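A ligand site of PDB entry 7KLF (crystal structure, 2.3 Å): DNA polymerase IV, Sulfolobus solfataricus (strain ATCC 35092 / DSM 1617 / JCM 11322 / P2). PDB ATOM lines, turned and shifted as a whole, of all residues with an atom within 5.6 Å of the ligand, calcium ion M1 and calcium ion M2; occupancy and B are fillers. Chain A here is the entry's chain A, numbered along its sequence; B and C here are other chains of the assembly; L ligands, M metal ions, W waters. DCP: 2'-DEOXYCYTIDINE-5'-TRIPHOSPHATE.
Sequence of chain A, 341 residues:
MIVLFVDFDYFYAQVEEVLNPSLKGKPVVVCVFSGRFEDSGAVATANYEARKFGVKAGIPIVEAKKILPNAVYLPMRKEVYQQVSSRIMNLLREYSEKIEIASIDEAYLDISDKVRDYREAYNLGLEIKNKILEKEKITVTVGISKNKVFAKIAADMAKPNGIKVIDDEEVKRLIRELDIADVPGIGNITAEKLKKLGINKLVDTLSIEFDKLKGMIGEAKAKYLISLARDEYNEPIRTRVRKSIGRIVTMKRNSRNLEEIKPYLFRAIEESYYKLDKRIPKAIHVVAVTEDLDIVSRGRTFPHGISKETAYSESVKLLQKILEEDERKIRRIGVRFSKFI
Water W3 lies within hydrogen-bond range of OP1 of DC 13 of chain C (2.9 Å) and OD2 of Asp 7 of chain A (2.9 Å).
Water W4 lies within hydrogen-bond range of OH of Tyr 12 (2.6 Å) and O2 of the ligand (2.8 Å).
Water W1 bridges OD1 of Asp 9 and O of Asp 7 of chain A.
N1 of the ligand sits close to O of Ala 44, at 3.5 Å.
Residues that only touch the ligand: Asp 9 (3.4 Å), Ala 57 (3.95 Å) and DG 7 of chain B (3.9 Å).
Hydrophobic or aromatic side chains within 4 Å of the ligand: Phe 11, Tyr 12, Ala 44, Tyr 48 and Ala 57.
16 residues have an atom within 4 Å of the ligand: Asp 7 of chain A, Phe 8, Asp 9, Tyr 10, Phe 11, Tyr 12, Ala 44, Thr 45, Tyr 48, Arg 51, Ala 57, Asp 105, Lys 159, DG 6 of chain B, DG 7 of chain B and DC 13 of chain C.
The nearest printed residue that does not touch the ligand is Ile 104 (4.5 Å).
Calcium ion M1 is bound by OE2 of Glu 106 (2.4 Å), water W3 (2.5 Å) and O2A of the ligand (2.6 Å).
Slightly farther from calcium ion M1 lies the side-chain carboxylate (OD1) of Asp 105 (2.9 Å).
Slightly farther from calcium ion M1 lies the side-chain carboxylate (OD1) of Asp 7 of chain A (3.0 Å).
Three residues have an atom within 4 Å of calcium ion M2: Asp 7 of chain A, Phe 8 and Asp 105.
The nearest printed residue that does not touch calcium ion M2 is Asp 9 (4.4 Å).
The side-chain carboxylate (OD2) of Asp 7 of chain A is in salt-bridge range of the side-chain amino group (NZ) of Lys 159, at 3.2 Å.
The side-chain hydroxyl of Ser 103 lies within hydrogen-bond range of the side-chain carboxylate of Asp 105 (3.3 Å).
The side-chain hydroxyl (OG1) of Thr 45 sits at hydrogen-bond distance from the guanidinium group (NH2) of Arg 51, 3.2 Å away.
NH2 of Arg 51 is in hydrogen-bond range of O of Ala 46, 3.0 Å away.
O2 of DC 13 of chain C sits close to N2 of DG 7 of chain B (2.6 Å).
The side-chain hydroxyl of Ser 103 is in hydrogen-bond range of O3' of DC 13 of chain C, at 2.9 Å.
OG1 of Thr 45 sits at hydrogen-bond distance from O1B of the ligand, at 2.5 Å.
The backbone NH (N) of Tyr 10 sits at hydrogen-bond distance from an oxygen (O3G) of the ligand, at 2.6 Å.
A nitrogen (N4) of the ligand sits at hydrogen-bond distance from O6 of DG 6 of chain B (2.9 Å).
The guanidinium group of Arg 51 lies within salt-bridge range of an oxygen (O1G) of the ligand (2.7 Å).
OH of Tyr 48 sits at hydrogen-bond distance from O3G of the ligand (2.8 Å).
The side-chain amino group (NZ) of Lys 159 sits close to an oxygen (O2G) of the ligand.
An oxygen (O3') of the ligand lies within hydrogen-bond range of the backbone NH (N) of Tyr 12 (3.1 Å).
N4 of DC 13 of chain C lies within hydrogen-bond range of a nitrogen (N4) of the ligand, 3.3 Å away.
An oxygen (O2B) of the ligand sits close to the backbone NH (N) of Phe 11, at 3.4 Å.
C3' of DC 13 of chain C touches calcium ion M1, at 3.7 Å.
Four residues have an atom within 4 Å of calcium ion M1: Asp 7 of chain A, Asp 105, Glu 106 and DC 13 of chain C.
The nearest printed residue that does not touch calcium ion M1 is Ser 103 (4.6 Å).
Calcium ion M2 is bound by OD1 of Asp 7 of chain A (2.3 Å), O of Phe 8 (2.3 Å), O2A of the ligand (2.3 Å), O2B of the ligand (2.3 Å), O2G of the ligand (2.4 Å) and OD2 of Asp 105 (2.5 Å).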
ATOM      1  N   PHE A   5      20.673  21.005  -2.280  1.00  0.00           N
ATOM      2  CA  PHE A   5      19.311  20.488  -2.250  1.00  0.00           C
ATOM      3  C   PHE A   5      19.272  19.136  -2.957  1.00  0.00           C
ATOM      4  O   PHE A   5      19.826  18.985  -4.043  1.00  0.00           O
ATOM      5  CB  PHE A   5      18.339  21.471  -2.916  1.00  0.00           C
ATOM      6  CG  PHE A   5      16.951  20.949  -3.082  1.00  0.00           C
ATOM      7  CD1 PHE A   5      16.116  20.780  -1.991  1.00  0.00           C
ATOM      8  CD2 PHE A   5      16.460  20.633  -4.342  1.00  0.00           C
ATOM      9  CE1 PHE A   5      14.827  20.310  -2.155  1.00  0.00           C
ATOM     10  CE2 PHE A   5      15.173  20.162  -4.515  1.00  0.00           C
ATOM     11  CZ  PHE A   5      14.356  20.000  -3.422  1.00  0.00           C
ATOM     12  N   ASP A   7      16.796  15.913  -4.290  1.00  0.00           N
ATOM     13  CA  ASP A   7      15.443  15.576  -4.717  1.00  0.00           C
ATOM     14  C   ASP A   7      15.468  14.205  -5.351  1.00  0.00           C
ATOM     15  O   ASP A   7      16.131  14.009  -6.375  1.00  0.00           O
ATOM     16  CB  ASP A   7      14.910  16.630  -5.691  1.00  0.00           C
ATOM     17  CG  ASP A   7      13.410  16.561  -5.876  1.00  0.00           C
ATOM     18  OD1 ASP A   7      12.832  15.468  -5.705  1.00  0.00           O
ATOM     19  OD2 ASP A   7      12.798  17.609  -6.182  1.00  0.00           O
ATOM     20  N   PHE A   8      14.753  13.245  -4.755  1.00  0.00           N
ATOM     21  CA  PHE A   8      14.814  11.866  -5.230  1.00  0.00           C
ATOM     22  C   PHE A   8      14.022  11.728  -6.522  1.00  0.00           C
ATOM     23  O   PHE A   8      12.894  12.201  -6.631  1.00  0.00           O
ATOM     24  CB  PHE A   8      14.270  10.896  -4.178  1.00  0.00           C
ATOM     25  CG  PHE A   8      14.843  11.080  -2.784  1.00  0.00           C
ATOM     26  CD1 PHE A   8      16.022  11.794  -2.574  1.00  0.00           C
ATOM     27  CD2 PHE A   8      14.213  10.505  -1.691  1.00  0.00           C
ATOM     28  CE1 PHE A   8      16.525  11.945  -1.291  1.00  0.00           C
ATOM     29  CE2 PHE A   8      14.718  10.655  -0.418  1.00  0.00           C
ATOM     30  CZ  PHE A   8      15.871  11.380  -0.214  1.00  0.00           C
ATOM     31  N   ASP A   9      14.618  11.062  -7.515  1.00  0.00           N
ATOM     32  CA  ASP A   9      13.988  10.933  -8.821  1.00  0.00           C
ATOM     33  C   ASP A   9      12.819   9.954  -8.767  1.00  0.00           C
ATOM     34  O   ASP A   9      12.950   8.852  -8.223  1.00  0.00           O
ATOM     35  CB  ASP A   9      15.005  10.476  -9.859  1.00  0.00           C
ATOM     36  CG  ASP A   9      16.168  11.442  -9.995  1.00  0.00           C
ATOM     37  OD1 ASP A   9      15.937  12.662  -9.933  1.00  0.00           O
ATOM     38  OD2 ASP A   9      17.313  10.970 -10.167  1.00  0.00           O
ATOM     39  N   TYR A  10      11.681  10.355  -9.371  1.00  0.00           N
ATOM     40  CA  TYR A  10      10.432   9.600  -9.427  1.00  0.00           C
ATOM     41  C   TYR A  10      10.298   8.614  -8.275  1.00  0.00           C
ATOM     42  O   TYR A  10      10.218   7.401  -8.480  1.00  0.00           O
ATOM     43  CB  TYR A  10      10.283   8.898 -10.786  1.00  0.00           C
ATOM     44  CG  TYR A  10      11.378   7.919 -11.176  1.00  0.00           C
ATOM     45  CD1 TYR A  10      12.645   8.361 -11.553  1.00  0.00           C
ATOM     46  CD2 TYR A  10      11.144   6.547 -11.203  1.00  0.00           C
ATOM     47  CE1 TYR A  10      13.645   7.467 -11.914  1.00  0.00           C
ATOM     48  CE2 TYR A  10      12.126   5.646 -11.567  1.00  0.00           C
ATOM     49  CZ  TYR A  10      13.376   6.117 -11.918  1.00  0.00           C
ATOM     50  OH  TYR A  10      14.363   5.229 -12.282  1.00  0.00           O
ATOM     51  N   PHE A  11      10.231   9.146  -7.052  1.00  0.00           N
ATOM     52  CA  PHE A  11      10.605   8.371  -5.869  1.00  0.00           C
ATOM     53  C   PHE A  11       9.749   7.132  -5.694  1.00  0.00           C
ATOM     54  O   PHE A  11      10.283   6.017  -5.570  1.00  0.00           O
ATOM     55  CB  PHE A  11      10.526   9.259  -4.622  1.00  0.00           C
ATOM     56  CG  PHE A  11      11.037   8.580  -3.383  1.00  0.00           C
ATOM     57  CD1 PHE A  11      12.307   8.011  -3.365  1.00  0.00           C
ATOM     58  CD2 PHE A  11      10.265   8.531  -2.238  1.00  0.00           C
ATOM     59  CE1 PHE A  11      12.776   7.388  -2.228  1.00  0.00           C
ATOM     60  CE2 PHE A  11      10.745   7.903  -1.089  1.00  0.00           C
ATOM     61  CZ  PHE A  11      11.996   7.334  -1.095  1.00  0.00           C
ATOM     62  N   TYR A  12       8.421   7.282  -5.663  1.00  0.00           N
ATOM     63  CA  TYR A  12       7.557   6.139  -5.404  1.00  0.00           C
ATOM     64  C   TYR A  12       7.748   5.060  -6.468  1.00  0.00           C
ATOM     65  O   TYR A  12       7.847   3.871  -6.146  1.00  0.00           O
ATOM     66  CB  TYR A  12       6.088   6.561  -5.344  1.00  0.00           C
ATOM     67  CG  TYR A  12       5.698   7.424  -4.157  1.00  0.00           C
ATOM     68  CD1 TYR A  12       6.653   7.871  -3.245  1.00  0.00           C
ATOM     69  CD2 TYR A  12       4.380   7.777  -3.944  1.00  0.00           C
ATOM     70  CE1 TYR A  12       6.297   8.667  -2.170  1.00  0.00           C
ATOM     71  CE2 TYR A  12       4.006   8.565  -2.871  1.00  0.00           C
ATOM     72  CZ  TYR A  12       4.969   9.001  -1.988  1.00  0.00           C
ATOM     73  OH  TYR A  12       4.605   9.792  -0.924  1.00  0.00           O
ATOM     74  N   ALA A  13       7.796   5.462  -7.737  1.00  0.00           N
ATOM     75  CA  ALA A  13       8.016   4.492  -8.803  1.00  0.00           C
ATOM     76  C   ALA A  13       9.399   3.861  -8.701  1.00  0.00           C
ATOM     77  O   ALA A  13       9.548   2.644  -8.888  1.00  0.00           O
ATOM     78  CB  ALA A  13       7.826   5.153 -10.170  1.00  0.00           C
ATOM     79  N   VAL A  43      -3.274   9.240  -9.897  1.00  0.00           N
ATOM     80  CA  VAL A  43      -1.901   8.781 -10.013  1.00  0.00           C
ATOM     81  C   VAL A  43      -1.054   9.555  -9.019  1.00  0.00           C
ATOM     82  O   VAL A  43      -1.055  10.795  -9.022  1.00  0.00           O
ATOM     83  CB  VAL A  43      -1.363   8.958 -11.438  1.00  0.00           C
ATOM     84  CG1 VAL A  43       0.128   8.665 -11.494  1.00  0.00           C
ATOM     85  CG2 VAL A  43      -2.135   8.077 -12.412  1.00  0.00           C
ATOM     86  N   ALA A  44      -0.331   8.836  -8.148  1.00  0.00           N
ATOM     87  CA  ALA A  44       0.587   9.496  -7.236  1.00  0.00           C
ATOM     88  C   ALA A  44       1.836   9.969  -7.974  1.00  0.00           C
ATOM     89  O   ALA A  44       2.279  11.109  -7.795  1.00  0.00           O
ATOM     90  CB  ALA A  44       0.962   8.553  -6.093  1.00  0.00           C
ATOM     91  N   THR A  45       2.406   9.107  -8.816  1.00  0.00           N
ATOM     92  CA  THR A  45       3.527   9.457  -9.678  1.00  0.00           C
ATOM     93  C   THR A  45       3.732   8.318 -10.664  1.00  0.00           C
ATOM     94  O   THR A  45       3.158   7.231 -10.534  1.00  0.00           O
ATOM     95  CB  THR A  45       4.812   9.707  -8.881  1.00  0.00           C
ATOM     96  OG1 THR A  45       5.823  10.239  -9.754  1.00  0.00           O
ATOM     97  CG2 THR A  45       5.312   8.414  -8.282  1.00  0.00           C
ATOM     98  N   ALA A  46       4.583   8.572 -11.657  1.00  0.00           N
ATOM     99  CA  ALA A  46       4.949   7.565 -12.635  1.00  0.00           C
ATOM    100  C   ALA A  46       6.401   7.785 -13.037  1.00  0.00           C
ATOM    101  O   ALA A  46       6.910   8.914 -12.978  1.00  0.00           O
ATOM    102  CB  ALA A  46       4.048   7.617 -13.876  1.00  0.00           C
ATOM    103  N   TYR A  48       9.643   7.897 -15.743  1.00  0.00           N
ATOM    104  CA  TYR A  48       9.748   8.711 -16.950  1.00  0.00           C
ATOM    105  C   TYR A  48       9.324   7.954 -18.209  1.00  0.00           C
ATOM    106  O   TYR A  48       8.924   8.594 -19.183  1.00  0.00           O
ATOM    107  CB  TYR A  48      11.171   9.249 -17.094  1.00  0.00           C
ATOM    108  CG  TYR A  48      11.502  10.290 -16.032  1.00  0.00           C
ATOM    109  CD1 TYR A  48      11.235  11.631 -16.249  1.00  0.00           C
ATOM    110  CD2 TYR A  48      12.055   9.907 -14.816  1.00  0.00           C
ATOM    111  CE1 TYR A  48      11.522  12.575 -15.290  1.00  0.00           C
ATOM    112  CE2 TYR A  48      12.355  10.846 -13.854  1.00  0.00           C
ATOM    113  CZ  TYR A  48      12.082  12.182 -14.092  1.00  0.00           C
ATOM    114  OH  TYR A  48      12.375  13.116 -13.142  1.00  0.00           O
ATOM    115  N   ARG A  51       5.784   8.794 -17.853  1.00  0.00           N
ATOM    116  CA  ARG A  51       5.574  10.234 -17.833  1.00  0.00           C
ATOM    117  C   ARG A  51       5.798  10.870 -19.191  1.00  0.00           C
ATOM    118  O   ARG A  51       5.235  11.944 -19.449  1.00  0.00           O
ATOM    119  CB  ARG A  51       6.495  10.871 -16.788  1.00  0.00           C
ATOM    120  CG  ARG A  51       6.061  12.258 -16.335  1.00  0.00           C
ATOM    121  CD  ARG A  51       7.012  12.829 -15.300  1.00  0.00           C
ATOM    122  NE  ARG A  51       7.031  12.047 -14.065  1.00  0.00           N
ATOM    123  CZ  ARG A  51       7.768  12.362 -12.997  1.00  0.00           C
ATOM    124  NH1 ARG A  51       8.555  13.429 -13.020  1.00  0.00           N
ATOM    125  NH2 ARG A  51       7.724  11.599 -11.916  1.00  0.00           N
ATOM    126  N   ALA A  57       1.531  12.860 -12.287  1.00  0.00           N
ATOM    127  CA  ALA A  57       0.822  12.875 -11.014  1.00  0.00           C
ATOM    128  C   ALA A  57      -0.437  13.724 -11.090  1.00  0.00           C
ATOM    129  O   ALA A  57      -0.460  14.781 -11.724  1.00  0.00           O
ATOM    130  CB  ALA A  57       1.745  13.412  -9.911  1.00  0.00           C
ATOM    131  N   GLY A  58      -1.507  13.246 -10.443  1.00  0.00           N
ATOM    132  CA  GLY A  58      -2.740  13.984 -10.294  1.00  0.00           C
ATOM    133  C   GLY A  58      -3.859  13.544 -11.223  1.00  0.00           C
ATOM    134  O   GLY A  58      -5.031  13.682 -10.860  1.00  0.00           O
ATOM    135  N   MET A  76      -0.185   2.408  -4.170  1.00  0.00           N
ATOM    136  CA  MET A  76       0.785   3.170  -3.389  1.00  0.00           C
ATOM    137  C   MET A  76       1.062   2.474  -2.055  1.00  0.00           C
ATOM    138  O   MET A  76       0.134   2.190  -1.287  1.00  0.00           O
ATOM    139  CB  MET A  76       0.269   4.591  -3.155  1.00  0.00           C
ATOM    140  CG  MET A  76       1.280   5.497  -2.479  1.00  0.00           C
ATOM    141  SD  MET A  76       0.650   7.156  -2.158  1.00  0.00           S
ATOM    142  CE  MET A  76      -0.664   6.802  -0.992  1.00  0.00           C
ATOM    143  N   SER A 103      10.237  17.180   2.635  1.00  0.00           N
ATOM    144  CA  SER A 103       9.133  16.267   2.340  1.00  0.00           C
ATOM    145  C   SER A 103       9.692  14.851   2.337  1.00  0.00           C
ATOM    146  O   SER A 103      10.804  14.606   2.814  1.00  0.00           O
ATOM    147  CB  SER A 103       8.458  16.638   1.013  1.00  0.00           C
ATOM    148  OG  SER A 103       9.312  16.325  -0.083  1.00  0.00           O
ATOM    149  N   ILE A 104       8.908  13.912   1.782  1.00  0.00           N
ATOM    150  CA  ILE A 104       9.327  12.516   1.784  1.00  0.00           C
ATOM    151  C   ILE A 104      10.511  12.273   0.861  1.00  0.00           C
ATOM    152  O   ILE A 104      11.176  11.242   0.971  1.00  0.00           O
ATOM    153  CB  ILE A 104       8.126  11.627   1.400  1.00  0.00           C
ATOM    154  CG1 ILE A 104       8.389  10.164   1.777  1.00  0.00           C
ATOM    155  CG2 ILE A 104       7.818  11.755  -0.093  1.00  0.00           C
ATOM    156  CD1 ILE A 104       7.180   9.271   1.626  1.00  0.00           C
ATOM    157  N   ASP A 105      10.818  13.211  -0.046  1.00  0.00           N
ATOM    158  CA  ASP A 105      11.935  12.996  -0.962  1.00  0.00           C
ATOM    159  C   ASP A 105      12.745  14.261  -1.207  1.00  0.00           C
ATOM    160  O   ASP A 105      13.417  14.382  -2.241  1.00  0.00           O
ATOM    161  CB  ASP A 105      11.445  12.419  -2.295  1.00  0.00           C
ATOM    162  CG  ASP A 105      10.731  13.448  -3.155  1.00  0.00           C
ATOM    163  OD1 ASP A 105      10.088  14.363  -2.584  1.00  0.00           O
ATOM    164  OD2 ASP A 105      10.815  13.346  -4.395  1.00  0.00           O
ATOM    165  N   GLU A 106      12.714  15.213  -0.271  1.00  0.00           N
ATOM    166  CA  GLU A 106      13.454  16.461  -0.425  1.00  0.00           C
ATOM    167  C   GLU A 106      14.182  16.802   0.862  1.00  0.00           C
ATOM    168  O   GLU A 106      13.656  16.574   1.958  1.00  0.00           O
ATOM    169  CB  GLU A 106      12.520  17.619  -0.803  1.00  0.00           C
ATOM    170  CG  GLU A 106      11.810  17.454  -2.130  1.00  0.00           C
ATOM    171  CD  GLU A 106      11.065  18.695  -2.542  1.00  0.00           C
ATOM    172  OE1 GLU A 106      10.977  19.640  -1.727  1.00  0.00           O
ATOM    173  OE2 GLU A 106      10.567  18.748  -3.696  1.00  0.00           O
ATOM    174  N   LYS A 159      16.800  17.870 -13.578  1.00  0.00           N
ATOM    175  CA  LYS A 159      16.071  16.938 -12.732  1.00  0.00           C
ATOM    176  C   LYS A 159      16.498  15.478 -12.907  1.00  0.00           C
ATOM    177  O   LYS A 159      17.130  14.933 -12.002  1.00  0.00           O
ATOM    178  CB  LYS A 159      14.561  17.087 -12.965  1.00  0.00           C
ATOM    179  CG  LYS A 159      13.717  16.493 -11.846  1.00  0.00           C
ATOM    180  CD  LYS A 159      12.980  17.592 -11.089  1.00  0.00           C
ATOM    181  CE  LYS A 159      12.430  17.068  -9.774  1.00  0.00           C
ATOM    182  NZ  LYS A 159      11.519  18.039  -9.108  1.00  0.00           N
ATOM    183  P    DG B   6     -11.462   9.905  -6.130  1.00  0.00           P
ATOM    184  OP1  DG B   6     -12.211   8.952  -6.973  1.00  0.00           O
ATOM    185  OP2  DG B   6     -11.749   9.953  -4.678  1.00  0.00           O
ATOM    186  O5'  DG B   6      -9.901   9.583  -6.284  1.00  0.00           O
ATOM    187  C5'  DG B   6      -8.941  10.379  -5.619  1.00  0.00           C
ATOM    188  C4'  DG B   6      -8.136   9.534  -4.644  1.00  0.00           C
ATOM    189  O4'  DG B   6      -6.719   9.776  -4.860  1.00  0.00           O
ATOM    190  C3'  DG B   6      -8.357   9.861  -3.179  1.00  0.00           C
ATOM    191  O3'  DG B   6      -7.980   8.741  -2.379  1.00  0.00           O
ATOM    192  C2'  DG B   6      -7.415  11.033  -2.979  1.00  0.00           C
ATOM    193  C1'  DG B   6      -6.221  10.618  -3.839  1.00  0.00           C
ATOM    194  N9   DG B   6      -5.538  11.744  -4.482  1.00  0.00           N
ATOM    195  C8   DG B   6      -6.115  12.747  -5.216  1.00  0.00           C
ATOM    196  N7   DG B   6      -5.248  13.614  -5.678  1.00  0.00           N
ATOM    197  C5   DG B   6      -4.024  13.139  -5.228  1.00  0.00           C
ATOM    198  C6   DG B   6      -2.718  13.657  -5.410  1.00  0.00           C
ATOM    199  O6   DG B   6      -2.386  14.675  -6.034  1.00  0.00           O
ATOM    200  N1   DG B   6      -1.758  12.870  -4.779  1.00  0.00           N
ATOM    201  C2   DG B   6      -2.020  11.731  -4.055  1.00  0.00           C
ATOM    202  N2   DG B   6      -0.965  11.112  -3.521  1.00  0.00           N
ATOM    203  N3   DG B   6      -3.237  11.238  -3.879  1.00  0.00           N
ATOM    204  C4   DG B   6      -4.185  11.989  -4.485  1.00  0.00           C
ATOM    205  P    DG B   7      -8.459   8.646  -0.847  1.00  0.00           P
ATOM    206  OP1  DG B   7      -8.574   7.210  -0.505  1.00  0.00           O
ATOM    207  OP2  DG B   7      -9.612   9.550  -0.675  1.00  0.00           O
ATOM    208  O5'  DG B   7      -7.228   9.247  -0.032  1.00  0.00           O
ATOM    209  C5'  DG B   7      -6.000   8.534   0.019  1.00  0.00           C
ATOM    210  C4'  DG B   7      -4.889   9.399   0.573  1.00  0.00           C
ATOM    211  O4'  DG B   7      -4.534  10.424  -0.393  1.00  0.00           O
ATOM    212  C3'  DG B   7      -5.219  10.138   1.870  1.00  0.00           C
ATOM    213  O3'  DG B   7      -4.263   9.781   2.867  1.00  0.00           O
ATOM    214  C2'  DG B   7      -5.112  11.631   1.491  1.00  0.00           C
ATOM    215  C1'  DG B   7      -4.171  11.581   0.311  1.00  0.00           C
ATOM    216  N9   DG B   7      -4.270  12.724  -0.587  1.00  0.00           N
ATOM    217  C8   DG B   7      -5.418  13.274  -1.111  1.00  0.00           C
ATOM    218  N7   DG B   7      -5.196  14.293  -1.885  1.00  0.00           N
ATOM    219  C5   DG B   7      -3.809  14.432  -1.886  1.00  0.00           C
ATOM    220  C6   DG B   7      -2.984  15.362  -2.553  1.00  0.00           C
ATOM    221  O6   DG B   7      -3.310  16.293  -3.301  1.00  0.00           O
ATOM    222  N1   DG B   7      -1.637  15.143  -2.272  1.00  0.00           N
ATOM    223  C2   DG B   7      -1.151  14.147  -1.452  1.00  0.00           C
ATOM    224  N2   DG B   7       0.179  14.088  -1.307  1.00  0.00           N
ATOM    225  N3   DG B   7      -1.915  13.268  -0.829  1.00  0.00           N
ATOM    226  C4   DG B   7      -3.235  13.468  -1.094  1.00  0.00           C
ATOM    227  P    DC C  13       7.077  20.448  -5.158  1.00  0.00           P
ATOM    228  OP1  DC C  13       8.501  20.833  -5.231  1.00  0.00           O
ATOM    229  OP2  DC C  13       6.267  20.386  -6.397  1.00  0.00           O
ATOM    230  O5'  DC C  13       6.959  19.043  -4.422  1.00  0.00           O
ATOM    231  C5'  DC C  13       7.311  18.927  -3.044  1.00  0.00           C
ATOM    232  C4'  DC C  13       6.633  17.738  -2.406  1.00  0.00           C
ATOM    233  O4'  DC C  13       5.199  17.939  -2.395  1.00  0.00           O
ATOM    234  C3'  DC C  13       6.865  16.396  -3.119  1.00  0.00           C
ATOM    235  O3'  DC C  13       7.474  15.471  -2.223  1.00  0.00           O
ATOM    236  C2'  DC C  13       5.463  15.942  -3.546  1.00  0.00           C
ATOM    237  C1'  DC C  13       4.568  16.700  -2.579  1.00  0.00           C
ATOM    238  N1   DC C  13       3.186  16.919  -3.079  1.00  0.00           N
ATOM    239  C2   DC C  13       2.097  16.350  -2.410  1.00  0.00           C
ATOM    240  O2   DC C  13       2.307  15.658  -1.403  1.00  0.00           O
ATOM    241  N3   DC C  13       0.847  16.559  -2.887  1.00  0.00           N
ATOM    242  C4   DC C  13       0.665  17.316  -3.975  1.00  0.00           C
ATOM    243  N4   DC C  13      -0.592  17.498  -4.401  1.00  0.00           N
ATOM    244  C5   DC C  13       1.758  17.906  -4.666  1.00  0.00           C
ATOM    245  C6   DC C  13       2.990  17.689  -4.191  1.00  0.00           C
HETATM  246  N1  DCP L   1       3.298  12.752  -4.931  1.00  0.00           N
HETATM  247  C2  DCP L   1       1.935  12.526  -4.677  1.00  0.00           C
HETATM  248  N3  DCP L   1       1.004  13.346  -5.223  1.00  0.00           N
HETATM  249  C4  DCP L   1       1.375  14.379  -6.014  1.00  0.00           C
HETATM  250  C5  DCP L   1       2.716  14.606  -6.273  1.00  0.00           C
HETATM  251  C6  DCP L   1       3.675  13.767  -5.710  1.00  0.00           C
HETATM  252  O2  DCP L   1       1.580  11.577  -3.950  1.00  0.00           O
HETATM  253  N4  DCP L   1       0.434  15.196  -6.553  1.00  0.00           N
HETATM  254  C1' DCP L   1       4.310  11.860  -4.356  1.00  0.00           C
HETATM  255  C2' DCP L   1       4.826  10.921  -5.435  1.00  0.00           C
HETATM  256  C3' DCP L   1       6.277  11.287  -5.644  1.00  0.00           C
HETATM  257  C4' DCP L   1       6.661  12.091  -4.405  1.00  0.00           C
HETATM  258  O4' DCP L   1       5.424  12.616  -3.885  1.00  0.00           O
HETATM  259  O3' DCP L   1       7.096  10.123  -5.773  1.00  0.00           O
HETATM  260  C5' DCP L   1       7.585  13.232  -4.775  1.00  0.00           C
HETATM  261  O5' DCP L   1       7.000  13.934  -5.866  1.00  0.00           O
HETATM  262  PA  DCP L   1       7.889  14.861  -6.827  1.00  0.00           P
HETATM  263  O1A DCP L   1       7.136  16.158  -7.041  1.00  0.00           O
HETATM  264  O2A DCP L   1       9.313  14.908  -6.338  1.00  0.00           O
HETATM  265  O3A DCP L   1       7.790  14.023  -8.209  1.00  0.00           O
HETATM  266  PB  DCP L   1       8.632  12.674  -8.484  1.00  0.00           P
HETATM  267  O1B DCP L   1       7.642  11.545  -8.624  1.00  0.00           O
HETATM  268  O2B DCP L   1       9.772  12.509  -7.510  1.00  0.00           O
HETATM  269  O3B DCP L   1       9.185  13.014  -9.959  1.00  0.00           O
HETATM  270  PG  DCP L   1      10.576  13.787 -10.196  1.00  0.00           P
HETATM  271  O1G DCP L   1      10.292  14.685 -11.382  1.00  0.00           O
HETATM  272  O2G DCP L   1      10.823  14.540  -8.915  1.00  0.00           O
HETATM  273  O3G DCP L   1      11.566  12.683 -10.473  1.00  0.00           O
HETATM  274 CA    CA M   1      10.305  16.501  -4.552  1.00  0.00          CA
HETATM  275 CA    CA M   2      11.409  13.960  -6.695  1.00  0.00          CA
HETATM  276  O   HOH W   1      14.248  14.489  -8.654  1.00  0.00           O
HETATM  277  O   HOH W   2       1.155  17.080  -8.532  1.00  0.00           O
HETATM  278  O   HOH W   3      10.017  18.488  -5.965  1.00  0.00           O
HETATM  279  O   HOH W   4       2.303  10.963  -1.348  1.00  0.00           O
